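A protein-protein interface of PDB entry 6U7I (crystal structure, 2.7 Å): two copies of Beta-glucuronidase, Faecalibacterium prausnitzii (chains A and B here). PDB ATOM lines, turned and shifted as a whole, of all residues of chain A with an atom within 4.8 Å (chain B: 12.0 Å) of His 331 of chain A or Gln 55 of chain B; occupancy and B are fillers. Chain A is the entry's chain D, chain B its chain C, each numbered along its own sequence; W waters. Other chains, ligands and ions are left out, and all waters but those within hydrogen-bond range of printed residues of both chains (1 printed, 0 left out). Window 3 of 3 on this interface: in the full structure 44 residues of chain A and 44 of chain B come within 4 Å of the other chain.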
ATOM      1  N   VAL A 327     -17.266 -29.413  -2.170  1.00  0.00           N
ATOM      2  CA  VAL A 327     -17.036 -30.775  -2.657  1.00  0.00           C
ATOM      3  C   VAL A 327     -15.897 -30.826  -3.663  1.00  0.00           C
ATOM      4  O   VAL A 327     -15.191 -31.836  -3.785  1.00  0.00           O
ATOM      5  CB  VAL A 327     -18.328 -31.348  -3.268  1.00  0.00           C
ATOM      6  CG1 VAL A 327     -18.157 -32.821  -3.509  1.00  0.00           C
ATOM      7  CG2 VAL A 327     -19.478 -31.127  -2.321  1.00  0.00           C
ATOM      8  N   ASN A 328     -15.726 -29.761  -4.434  1.00  0.00           N
ATOM      9  CA  ASN A 328     -14.600 -29.726  -5.350  1.00  0.00           C
ATOM     10  C   ASN A 328     -13.304 -29.396  -4.609  1.00  0.00           C
ATOM     11  O   ASN A 328     -12.242 -29.946  -4.928  1.00  0.00           O
ATOM     12  CB  ASN A 328     -14.896 -28.734  -6.462  1.00  0.00           C
ATOM     13  CG  ASN A 328     -15.865 -29.292  -7.507  1.00  0.00           C
ATOM     14  OD1 ASN A 328     -15.750 -30.448  -7.934  1.00  0.00           O
ATOM     15  ND2 ASN A 328     -16.796 -28.457  -7.935  1.00  0.00           N
ATOM     16  N   LEU A 329     -13.373 -28.527  -3.594  1.00  0.00           N
ATOM     17  CA  LEU A 329     -12.221 -28.366  -2.709  1.00  0.00           C
ATOM     18  C   LEU A 329     -11.952 -29.640  -1.916  1.00  0.00           C
ATOM     19  O   LEU A 329     -10.808 -29.920  -1.547  1.00  0.00           O
ATOM     20  CB  LEU A 329     -12.422 -27.184  -1.756  1.00  0.00           C
ATOM     21  CG  LEU A 329     -12.202 -25.802  -2.380  1.00  0.00           C
ATOM     22  CD1 LEU A 329     -12.851 -24.687  -1.567  1.00  0.00           C
ATOM     23  CD2 LEU A 329     -10.707 -25.558  -2.554  1.00  0.00           C
ATOM     24  N   ILE A 330     -12.982 -30.436  -1.670  1.00  0.00           N
ATOM     25  CA  ILE A 330     -12.774 -31.692  -0.974  1.00  0.00           C
ATOM     26  C   ILE A 330     -12.037 -32.684  -1.875  1.00  0.00           C
ATOM     27  O   ILE A 330     -11.153 -33.412  -1.419  1.00  0.00           O
ATOM     28  CB  ILE A 330     -14.132 -32.188  -0.443  1.00  0.00           C
ATOM     29  CG1 ILE A 330     -14.613 -31.142   0.582  1.00  0.00           C
ATOM     30  CG2 ILE A 330     -14.030 -33.579   0.153  1.00  0.00           C
ATOM     31  CD1 ILE A 330     -15.833 -31.459   1.402  1.00  0.00           C
ATOM     32  N   HIS A 331     -12.322 -32.680  -3.178  1.00  0.00           N
ATOM     33  CA  HIS A 331     -11.531 -33.504  -4.098  1.00  0.00           C
ATOM     34  C   HIS A 331     -10.107 -32.977  -4.240  1.00  0.00           C
ATOM     35  O   HIS A 331      -9.132 -33.735  -4.140  1.00  0.00           O
ATOM     36  CB  HIS A 331     -12.195 -33.548  -5.468  1.00  0.00           C
ATOM     37  CG  HIS A 331     -13.493 -34.282  -5.485  1.00  0.00           C
ATOM     38  ND1 HIS A 331     -13.736 -35.380  -4.689  1.00  0.00           N
ATOM     39  CD2 HIS A 331     -14.624 -34.068  -6.194  1.00  0.00           C
ATOM     40  CE1 HIS A 331     -14.965 -35.806  -4.904  1.00  0.00           C
ATOM     41  NE2 HIS A 331     -15.524 -35.025  -5.812  1.00  0.00           N
ATOM     42  N   TRP A 332      -9.980 -31.681  -4.515  1.00  0.00           N
ATOM     43  CA  TRP A 332      -8.676 -31.038  -4.629  1.00  0.00           C
ATOM     44  C   TRP A 332      -7.772 -31.345  -3.444  1.00  0.00           C
ATOM     45  O   TRP A 332      -6.550 -31.409  -3.602  1.00  0.00           O
ATOM     46  CB  TRP A 332      -8.879 -29.535  -4.769  1.00  0.00           C
ATOM     47  CG  TRP A 332      -7.654 -28.714  -4.707  1.00  0.00           C
ATOM     48  CD1 TRP A 332      -6.781 -28.469  -5.718  1.00  0.00           C
ATOM     49  CD2 TRP A 332      -7.170 -27.990  -3.573  1.00  0.00           C
ATOM     50  NE1 TRP A 332      -5.769 -27.651  -5.284  1.00  0.00           N
ATOM     51  CE2 TRP A 332      -5.990 -27.337  -3.971  1.00  0.00           C
ATOM     52  CE3 TRP A 332      -7.615 -27.844  -2.253  1.00  0.00           C
ATOM     53  CZ2 TRP A 332      -5.261 -26.536  -3.109  1.00  0.00           C
ATOM     54  CZ3 TRP A 332      -6.895 -27.050  -1.401  1.00  0.00           C
ATOM     55  CH2 TRP A 332      -5.726 -26.402  -1.833  1.00  0.00           C
ATOM     56  N   ALA A 333      -8.355 -31.553  -2.261  1.00  0.00           N
ATOM     57  CA  ALA A 333      -7.609 -31.849  -1.041  1.00  0.00           C
ATOM     58  C   ALA A 333      -7.145 -33.294  -0.945  1.00  0.00           C
ATOM     59  O   ALA A 333      -6.353 -33.602  -0.049  1.00  0.00           O
ATOM     60  CB  ALA A 333      -8.453 -31.529   0.189  1.00  0.00           C
ATOM     61  N   ASN A 334      -7.604 -34.170  -1.844  1.00  0.00           N
ATOM     62  CA  ASN A 334      -7.378 -35.615  -1.795  1.00  0.00           C
ATOM     63  C   ASN A 334      -8.089 -36.275  -0.623  1.00  0.00           C
ATOM     64  O   ASN A 334      -7.701 -37.366  -0.191  1.00  0.00           O
ATOM     65  CB  ASN A 334      -5.889 -35.945  -1.777  1.00  0.00           C
ATOM     66  CG  ASN A 334      -5.164 -35.324  -2.940  1.00  0.00           C
ATOM     67  OD1 ASN A 334      -5.652 -35.373  -4.080  1.00  0.00           O
ATOM     68  ND2 ASN A 334      -4.011 -34.705  -2.668  1.00  0.00           N
ATOM     69  N   ALA A 335      -9.136 -35.620  -0.121  1.00  0.00           N
ATOM     70  CA  ALA A 335     -10.013 -36.063   0.948  1.00  0.00           C
ATOM     71  C   ALA A 335     -11.159 -36.912   0.389  1.00  0.00           C
ATOM     72  O   ALA A 335     -11.556 -36.776  -0.769  1.00  0.00           O
ATOM     73  CB  ALA A 335     -10.571 -34.849   1.684  1.00  0.00           C
ATOM     74  N   GLU A 356     -20.770 -37.240  -6.111  1.00  0.00           N
ATOM     75  CA  GLU A 356     -19.347 -36.904  -6.158  1.00  0.00           C
ATOM     76  C   GLU A 356     -18.461 -38.002  -5.596  1.00  0.00           C
ATOM     77  O   GLU A 356     -17.285 -38.080  -5.958  1.00  0.00           O
ATOM     78  CB  GLU A 356     -19.114 -35.594  -5.425  1.00  0.00           C
ATOM     79  CG  GLU A 356     -19.424 -34.429  -6.327  1.00  0.00           C
ATOM     80  CD  GLU A 356     -18.731 -34.597  -7.652  1.00  0.00           C
ATOM     81  OE1 GLU A 356     -17.488 -34.464  -7.697  1.00  0.00           O
ATOM     82  OE2 GLU A 356     -19.422 -34.912  -8.645  1.00  0.00           O
ATOM     83  N   ILE A 358     -18.374 -39.233  -1.982  1.00  0.00           N
ATOM     84  CA  ILE A 358     -17.777 -38.755  -0.743  1.00  0.00           C
ATOM     85  C   ILE A 358     -18.480 -39.418   0.424  1.00  0.00           C
ATOM     86  O   ILE A 358     -19.697 -39.291   0.568  1.00  0.00           O
ATOM     87  CB  ILE A 358     -17.847 -37.224  -0.650  1.00  0.00           C
ATOM     88  CG1 ILE A 358     -16.822 -36.641  -1.612  1.00  0.00           C
ATOM     89  CG2 ILE A 358     -17.532 -36.747   0.751  1.00  0.00           C
ATOM     90  CD1 ILE A 358     -16.594 -35.196  -1.430  1.00  0.00           C
ATOM     91  N   PHE B  21     -22.733 -30.291 -16.472  1.00  0.00           N
ATOM     92  CA  PHE B  21     -21.906 -29.213 -17.003  1.00  0.00           C
ATOM     93  C   PHE B  21     -20.619 -29.755 -17.601  1.00  0.00           C
ATOM     94  O   PHE B  21     -19.971 -30.625 -17.014  1.00  0.00           O
ATOM     95  CB  PHE B  21     -21.590 -28.209 -15.898  1.00  0.00           C
ATOM     96  CG  PHE B  21     -20.564 -27.158 -16.270  1.00  0.00           C
ATOM     97  CD1 PHE B  21     -19.196 -27.430 -16.209  1.00  0.00           C
ATOM     98  CD2 PHE B  21     -20.964 -25.884 -16.605  1.00  0.00           C
ATOM     99  CE1 PHE B  21     -18.265 -26.465 -16.508  1.00  0.00           C
ATOM    100  CE2 PHE B  21     -20.031 -24.920 -16.903  1.00  0.00           C
ATOM    101  CZ  PHE B  21     -18.680 -25.207 -16.848  1.00  0.00           C
ATOM    102  N   LEU B  23     -17.035 -28.461 -19.998  1.00  0.00           N
ATOM    103  CA  LEU B  23     -16.290 -27.427 -20.695  1.00  0.00           C
ATOM    104  C   LEU B  23     -16.260 -27.759 -22.178  1.00  0.00           C
ATOM    105  O   LEU B  23     -16.322 -28.923 -22.570  1.00  0.00           O
ATOM    106  CB  LEU B  23     -14.864 -27.308 -20.157  1.00  0.00           C
ATOM    107  CG  LEU B  23     -14.588 -26.811 -18.730  1.00  0.00           C
ATOM    108  CD1 LEU B  23     -13.201 -27.273 -18.229  1.00  0.00           C
ATOM    109  CD2 LEU B  23     -14.718 -25.305 -18.647  1.00  0.00           C
ATOM    110  N   ASP B  39     -19.029 -36.887 -19.725  1.00  0.00           N
ATOM    111  CA  ASP B  39     -18.223 -36.551 -18.543  1.00  0.00           C
ATOM    112  C   ASP B  39     -18.702 -35.262 -17.900  1.00  0.00           C
ATOM    113  O   ASP B  39     -17.904 -34.410 -17.504  1.00  0.00           O
ATOM    114  CB  ASP B  39     -16.723 -36.431 -18.838  1.00  0.00           C
ATOM    115  CG  ASP B  39     -16.202 -37.501 -19.759  1.00  0.00           C
ATOM    116  OD1 ASP B  39     -16.296 -38.701 -19.412  1.00  0.00           O
ATOM    117  OD2 ASP B  39     -15.662 -37.124 -20.822  1.00  0.00           O
ATOM    118  N   ALA B  40     -20.013 -35.111 -17.784  1.00  0.00           N
ATOM    119  CA  ALA B  40     -20.509 -33.922 -17.133  1.00  0.00           C
ATOM    120  C   ALA B  40     -20.017 -33.864 -15.681  1.00  0.00           C
ATOM    121  O   ALA B  40     -19.402 -34.793 -15.156  1.00  0.00           O
ATOM    122  CB  ALA B  40     -22.029 -33.878 -17.213  1.00  0.00           C
ATOM    123  N   GLN B  41     -20.261 -32.727 -15.042  1.00  0.00           N
ATOM    124  CA  GLN B  41     -19.951 -32.537 -13.635  1.00  0.00           C
ATOM    125  C   GLN B  41     -21.020 -31.623 -13.069  1.00  0.00           C
ATOM    126  O   GLN B  41     -21.587 -30.808 -13.815  1.00  0.00           O
ATOM    127  CB  GLN B  41     -18.563 -31.924 -13.432  1.00  0.00           C
ATOM    128  CG  GLN B  41     -18.390 -30.559 -14.104  1.00  0.00           C
ATOM    129  CD  GLN B  41     -17.098 -29.868 -13.720  1.00  0.00           C
ATOM    130  OE1 GLN B  41     -16.960 -29.370 -12.599  1.00  0.00           O
ATOM    131  NE2 GLN B  41     -16.137 -29.841 -14.645  1.00  0.00           N
ATOM    132  N   PRO B  42     -21.336 -31.736 -11.777  1.00  0.00           N
ATOM    133  CA  PRO B  42     -22.403 -30.898 -11.220  1.00  0.00           C
ATOM    134  C   PRO B  42     -21.977 -29.442 -11.200  1.00  0.00           C
ATOM    135  O   PRO B  42     -20.803 -29.132 -10.994  1.00  0.00           O
ATOM    136  CB  PRO B  42     -22.606 -31.452  -9.805  1.00  0.00           C
ATOM    137  CG  PRO B  42     -21.401 -32.254  -9.499  1.00  0.00           C
ATOM    138  CD  PRO B  42     -20.776 -32.679 -10.797  1.00  0.00           C
ATOM    139  N   ILE B  43     -22.930 -28.546 -11.460  1.00  0.00           N
ATOM    140  CA  ILE B  43     -22.663 -27.107 -11.438  1.00  0.00           C
ATOM    141  C   ILE B  43     -23.928 -26.400 -10.992  1.00  0.00           C
ATOM    142  O   ILE B  43     -25.037 -26.788 -11.369  1.00  0.00           O
ATOM    143  CB  ILE B  43     -22.164 -26.593 -12.810  1.00  0.00           C
ATOM    144  CG1 ILE B  43     -21.146 -25.462 -12.634  1.00  0.00           C
ATOM    145  CG2 ILE B  43     -23.302 -26.160 -13.726  1.00  0.00           C
ATOM    146  CD1 ILE B  43     -19.761 -25.970 -12.311  1.00  0.00           C
ATOM    147  N   TYR B  49     -19.718 -19.998 -13.488  1.00  0.00           N
ATOM    148  CA  TYR B  49     -19.114 -21.314 -13.317  1.00  0.00           C
ATOM    149  C   TYR B  49     -17.690 -21.243 -12.762  1.00  0.00           C
ATOM    150  O   TYR B  49     -17.132 -22.282 -12.395  1.00  0.00           O
ATOM    151  CB  TYR B  49     -19.154 -22.119 -14.635  1.00  0.00           C
ATOM    152  CG  TYR B  49     -18.484 -21.488 -15.811  1.00  0.00           C
ATOM    153  CD1 TYR B  49     -17.097 -21.494 -15.938  1.00  0.00           C
ATOM    154  CD2 TYR B  49     -19.220 -20.870 -16.807  1.00  0.00           C
ATOM    155  CE1 TYR B  49     -16.469 -20.889 -17.035  1.00  0.00           C
ATOM    156  CE2 TYR B  49     -18.603 -20.279 -17.902  1.00  0.00           C
ATOM    157  CZ  TYR B  49     -17.239 -20.297 -18.009  1.00  0.00           C
ATOM    158  OH  TYR B  49     -16.635 -19.717 -19.082  1.00  0.00           O
ATOM    159  N   ASN B  50     -17.132 -20.039 -12.604  1.00  0.00           N
ATOM    160  CA  ASN B  50     -15.680 -19.878 -12.619  1.00  0.00           C
ATOM    161  C   ASN B  50     -15.049 -20.348 -11.323  1.00  0.00           C
ATOM    162  O   ASN B  50     -14.012 -21.025 -11.338  1.00  0.00           O
ATOM    163  CB  ASN B  50     -15.327 -18.417 -12.917  1.00  0.00           C
ATOM    164  CG  ASN B  50     -15.705 -18.017 -14.337  1.00  0.00           C
ATOM    165  OD1 ASN B  50     -16.713 -17.346 -14.569  1.00  0.00           O
ATOM    166  ND2 ASN B  50     -14.922 -18.472 -15.295  1.00  0.00           N
ATOM    167  N   ASP B  51     -15.677 -20.029 -10.195  1.00  0.00           N
ATOM    168  CA  ASP B  51     -15.146 -20.340  -8.875  1.00  0.00           C
ATOM    169  C   ASP B  51     -15.807 -21.557  -8.270  1.00  0.00           C
ATOM    170  O   ASP B  51     -15.931 -21.643  -7.053  1.00  0.00           O
ATOM    171  CB  ASP B  51     -15.316 -19.145  -7.944  1.00  0.00           C
ATOM    172  CG  ASP B  51     -14.737 -17.901  -8.526  1.00  0.00           C
ATOM    173  OD1 ASP B  51     -14.102 -18.015  -9.592  1.00  0.00           O
ATOM    174  OD2 ASP B  51     -14.916 -16.817  -7.944  1.00  0.00           O
ATOM    175  N   GLN B  52     -16.248 -22.500  -9.098  1.00  0.00           N
ATOM    176  CA  GLN B  52     -17.031 -23.620  -8.611  1.00  0.00           C
ATOM    177  C   GLN B  52     -16.283 -24.944  -8.610  1.00  0.00           C
ATOM    178  O   GLN B  52     -16.729 -25.879  -7.942  1.00  0.00           O
ATOM    179  CB  GLN B  52     -18.308 -23.768  -9.444  1.00  0.00           C
ATOM    180  CG  GLN B  52     -19.496 -22.988  -8.897  1.00  0.00           C
ATOM    181  CD  GLN B  52     -20.840 -23.545  -9.366  1.00  0.00           C
ATOM    182  OE1 GLN B  52     -21.174 -24.708  -9.108  1.00  0.00           O
ATOM    183  NE2 GLN B  52     -21.617 -22.707 -10.046  1.00  0.00           N
ATOM    184  N   ASN B  53     -15.171 -25.059  -9.334  1.00  0.00           N
ATOM    185  CA  ASN B  53     -14.382 -26.290  -9.304  1.00  0.00           C
ATOM    186  C   ASN B  53     -12.911 -25.907  -9.217  1.00  0.00           C
ATOM    187  O   ASN B  53     -12.277 -25.596 -10.230  1.00  0.00           O
ATOM    188  CB  ASN B  53     -14.646 -27.163 -10.517  1.00  0.00           C
ATOM    189  CG  ASN B  53     -14.067 -28.531 -10.360  1.00  0.00           C
ATOM    190  OD1 ASN B  53     -13.362 -28.796  -9.395  1.00  0.00           O
ATOM    191  ND2 ASN B  53     -14.346 -29.410 -11.304  1.00  0.00           N
ATOM    192  N   ASP B  54     -12.364 -25.946  -8.005  1.00  0.00           N
ATOM    193  CA  ASP B  54     -10.965 -25.608  -7.800  1.00  0.00           C
ATOM    194  C   ASP B  54     -10.064 -26.829  -7.843  1.00  0.00           C
ATOM    195  O   ASP B  54      -8.911 -26.751  -7.404  1.00  0.00           O
ATOM    196  CB  ASP B  54     -10.792 -24.855  -6.482  1.00  0.00           C
ATOM    197  CG  ASP B  54     -11.521 -23.535  -6.483  1.00  0.00           C
ATOM    198  OD1 ASP B  54     -11.054 -22.607  -7.200  1.00  0.00           O
ATOM    199  OD2 ASP B  54     -12.569 -23.439  -5.783  1.00  0.00           O
ATOM    200  N   GLN B  55     -10.562 -27.953  -8.368  1.00  0.00           N
ATOM    201  CA  GLN B  55      -9.691 -29.105  -8.584  1.00  0.00           C
ATOM    202  C   GLN B  55      -8.540 -28.759  -9.522  1.00  0.00           C
ATOM    203  O   GLN B  55      -7.417 -29.254  -9.358  1.00  0.00           O
ATOM    204  CB  GLN B  55     -10.492 -30.260  -9.143  1.00  0.00           C
ATOM    205  CG  GLN B  55     -11.233 -31.051  -8.109  1.00  0.00           C
ATOM    206  CD  GLN B  55     -11.842 -32.281  -8.722  1.00  0.00           C
ATOM    207  OE1 GLN B  55     -11.124 -33.190  -9.145  1.00  0.00           O
ATOM    208  NE2 GLN B  55     -13.172 -32.294  -8.835  1.00  0.00           N
ATOM    209  N   THR B  56      -8.816 -27.947 -10.534  1.00  0.00           N
ATOM    210  CA  THR B  56      -7.814 -27.310 -11.365  1.00  0.00           C
ATOM    211  C   THR B  56      -8.287 -25.897 -11.622  1.00  0.00           C
ATOM    212  O   THR B  56      -9.348 -25.478 -11.160  1.00  0.00           O
ATOM    213  CB  THR B  56      -7.579 -28.019 -12.708  1.00  0.00           C
ATOM    214  OG1 THR B  56      -8.638 -27.687 -13.609  1.00  0.00           O
ATOM    215  CG2 THR B  56      -7.442 -29.538 -12.548  1.00  0.00           C
ATOM    216  N   THR B  57      -7.495 -25.155 -12.370  1.00  0.00           N
ATOM    217  CA  THR B  57      -7.818 -23.779 -12.678  1.00  0.00           C
ATOM    218  C   THR B  57      -8.499 -23.663 -14.044  1.00  0.00           C
ATOM    219  O   THR B  57      -8.688 -22.556 -14.568  1.00  0.00           O
ATOM    220  CB  THR B  57      -6.535 -22.975 -12.572  1.00  0.00           C
ATOM    221  OG1 THR B  57      -6.833 -21.612 -12.256  1.00  0.00           O
ATOM    222  CG2 THR B  57      -5.723 -23.118 -13.852  1.00  0.00           C
ATOM    223  N   ALA B  58      -8.923 -24.803 -14.595  1.00  0.00           N
ATOM    224  CA  ALA B  58      -9.504 -24.857 -15.927  1.00  0.00           C
ATOM    225  C   ALA B  58     -10.840 -24.131 -15.981  1.00  0.00           C
ATOM    226  O   ALA B  58     -11.177 -23.506 -16.996  1.00  0.00           O
ATOM    227  CB  ALA B  58      -9.682 -26.318 -16.344  1.00  0.00           C
ATOM    228  N   LEU B  59     -11.634 -24.235 -14.913  1.00  0.00           N
ATOM    229  CA  LEU B  59     -12.906 -23.528 -14.906  1.00  0.00           C
ATOM    230  C   LEU B  59     -12.683 -22.026 -14.748  1.00  0.00           C
ATOM    231  O   LEU B  59     -13.290 -21.224 -15.462  1.00  0.00           O
ATOM    232  CB  LEU B  59     -13.821 -24.105 -13.810  1.00  0.00           C
ATOM    233  CG  LEU B  59     -15.024 -24.951 -14.309  1.00  0.00           C
ATOM    234  CD1 LEU B  59     -14.591 -26.222 -15.061  1.00  0.00           C
ATOM    235  CD2 LEU B  59     -16.014 -25.318 -13.207  1.00  0.00           C
ATOM    236  N   ARG B  60     -11.771 -21.635 -13.858  1.00  0.00           N
ATOM    237  CA  ARG B  60     -11.573 -20.222 -13.555  1.00  0.00           C
ATOM    238  C   ARG B  60     -11.095 -19.452 -14.772  1.00  0.00           C
ATOM    239  O   ARG B  60     -11.495 -18.303 -14.983  1.00  0.00           O
ATOM    240  CB  ARG B  60     -10.569 -20.069 -12.415  1.00  0.00           C
ATOM    241  CG  ARG B  60     -10.103 -18.649 -12.172  1.00  0.00           C
ATOM    242  CD  ARG B  60     -11.137 -17.841 -11.393  1.00  0.00           C
ATOM    243  NE  ARG B  60     -10.604 -16.551 -10.956  1.00  0.00           N
ATOM    244  CZ  ARG B  60     -11.269 -15.683 -10.202  1.00  0.00           C
ATOM    245  NH1 ARG B  60     -12.497 -15.956  -9.797  1.00  0.00           N
ATOM    246  NH2 ARG B  60     -10.707 -14.546  -9.855  1.00  0.00           N
ATOM    247  N   ARG B  61     -10.235 -20.064 -15.583  1.00  0.00           N
ATOM    248  CA  ARG B  61      -9.532 -19.358 -16.647  1.00  0.00           C
ATOM    249  C   ARG B  61      -9.996 -19.769 -18.035  1.00  0.00           C
ATOM    250  O   ARG B  61      -9.328 -19.443 -19.031  1.00  0.00           O
ATOM    251  CB  ARG B  61      -8.025 -19.581 -16.511  1.00  0.00           C
ATOM    252  CG  ARG B  61      -7.563 -19.628 -15.083  1.00  0.00           C
ATOM    253  CD  ARG B  61      -6.107 -19.322 -15.003  1.00  0.00           C
ATOM    254  NE  ARG B  61      -5.700 -18.966 -13.658  1.00  0.00           N
ATOM    255  CZ  ARG B  61      -4.478 -19.171 -13.190  1.00  0.00           C
ATOM    256  NH1 ARG B  61      -3.569 -19.744 -13.973  1.00  0.00           N
ATOM    257  NH2 ARG B  61      -4.181 -18.816 -11.948  1.00  0.00           N
HETATM  258  O   HOH W   1     -18.263 -29.670 -10.439  1.00  0.00           O
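Of the 20 printed residues of chain B, 5 touch a printed residue of chain A. Hydrophobic or aromatic side chains of chain B within 4 Å of the printed part of chain A: Pro 42. Along chain B the printed residues that touch a printed residue of chain A span positions 42 to 55. Among the printed residues, 8 pairs touch across the chains.
The side-chain amide oxygen of Asn 328 of chain A sits close to the side-chain amide oxygen of Asn 53 of chain B, 3.3 Å away. The side-chain amide nitrogen of Asn 328 of chain A is in hydrogen-bond range of the backbone carbonyl oxygen of Gln 52 of chain B (2.6 Å). NE2 of Gln 55 of chain B is in hydrogen-bond range of OD1 of Asn 328 of chain A (3.3 Å).
No residue of chain B comes within 4 Å of Val 327 of chain A. No residue of chain B comes within 4 Å of Ile 330 of chain A. His 331 of chain A touches one residue of chain B. Of the printed residues of chain B, Trp 332 of chain A touches Asp 54 and Gln 55. No residue of chain B comes within 4 Å of Ala 333 of chain A. No residue of chain B comes within 4 Å of Asn 334 of chain A. No residue of chain B comes within 4 Å of Ala 335 of chain A. Asp 39 of chain B touches none of the printed residues of chain A. Ile 43 of chain B touches none of the printed residues of chain A. Of the printed residues of chain A, Gln 52 of chain B touches Asn 328. Gln 55 of chain B touches just these residues of chain A: Asn 328 (3.3 Å), His 331 (3.5 Å) and Trp 332 (3.8 Å). The nearest residue of chain B that does not touch His 331 of chain A is Asn 53 of chain B (6.3 Å). The nearest printed residue of chain A that does not touch Gln 55 of chain B is Glu 356 of chain A (5.0 Å).
Water W1 lies within hydrogen-bond range of the side-chain amide oxygen of Gln 41 of chain B (2.5 Å), the backbone carbonyl oxygen of Pro 42 of chain B (2.7 Å) and the side-chain amide nitrogen of Asn 328 of chain A (3.1 Å).
No position is printed for both chains.
Leu 329 of chain A touches Asp 54 of chain B. His 331 of chain A touches Gln 55 of chain B. Asp 54 of chain B touches Trp 332 of chain A (O to CD1, 3.2 Å). Trp 332 of chain A touches Gln 55 of chain B (CD1 to O, 3.8 Å). CD of Pro 42 of chain B touches OE2 of Glu 356 of chain A (3.4 Å).
OE1 of Gln 41 of chain B lies within hydrogen-bond range of ND2 of Asn 53 of chain B. OE1 of Glu 356 of chain A is in hydrogen-bond range of NE2 of His 331 of chain A, at 2.8 Å. N of Gln 55 of chain B lies within hydrogen-bond range of OD1 of Asn 53 of chain B, 3.1 Å away.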
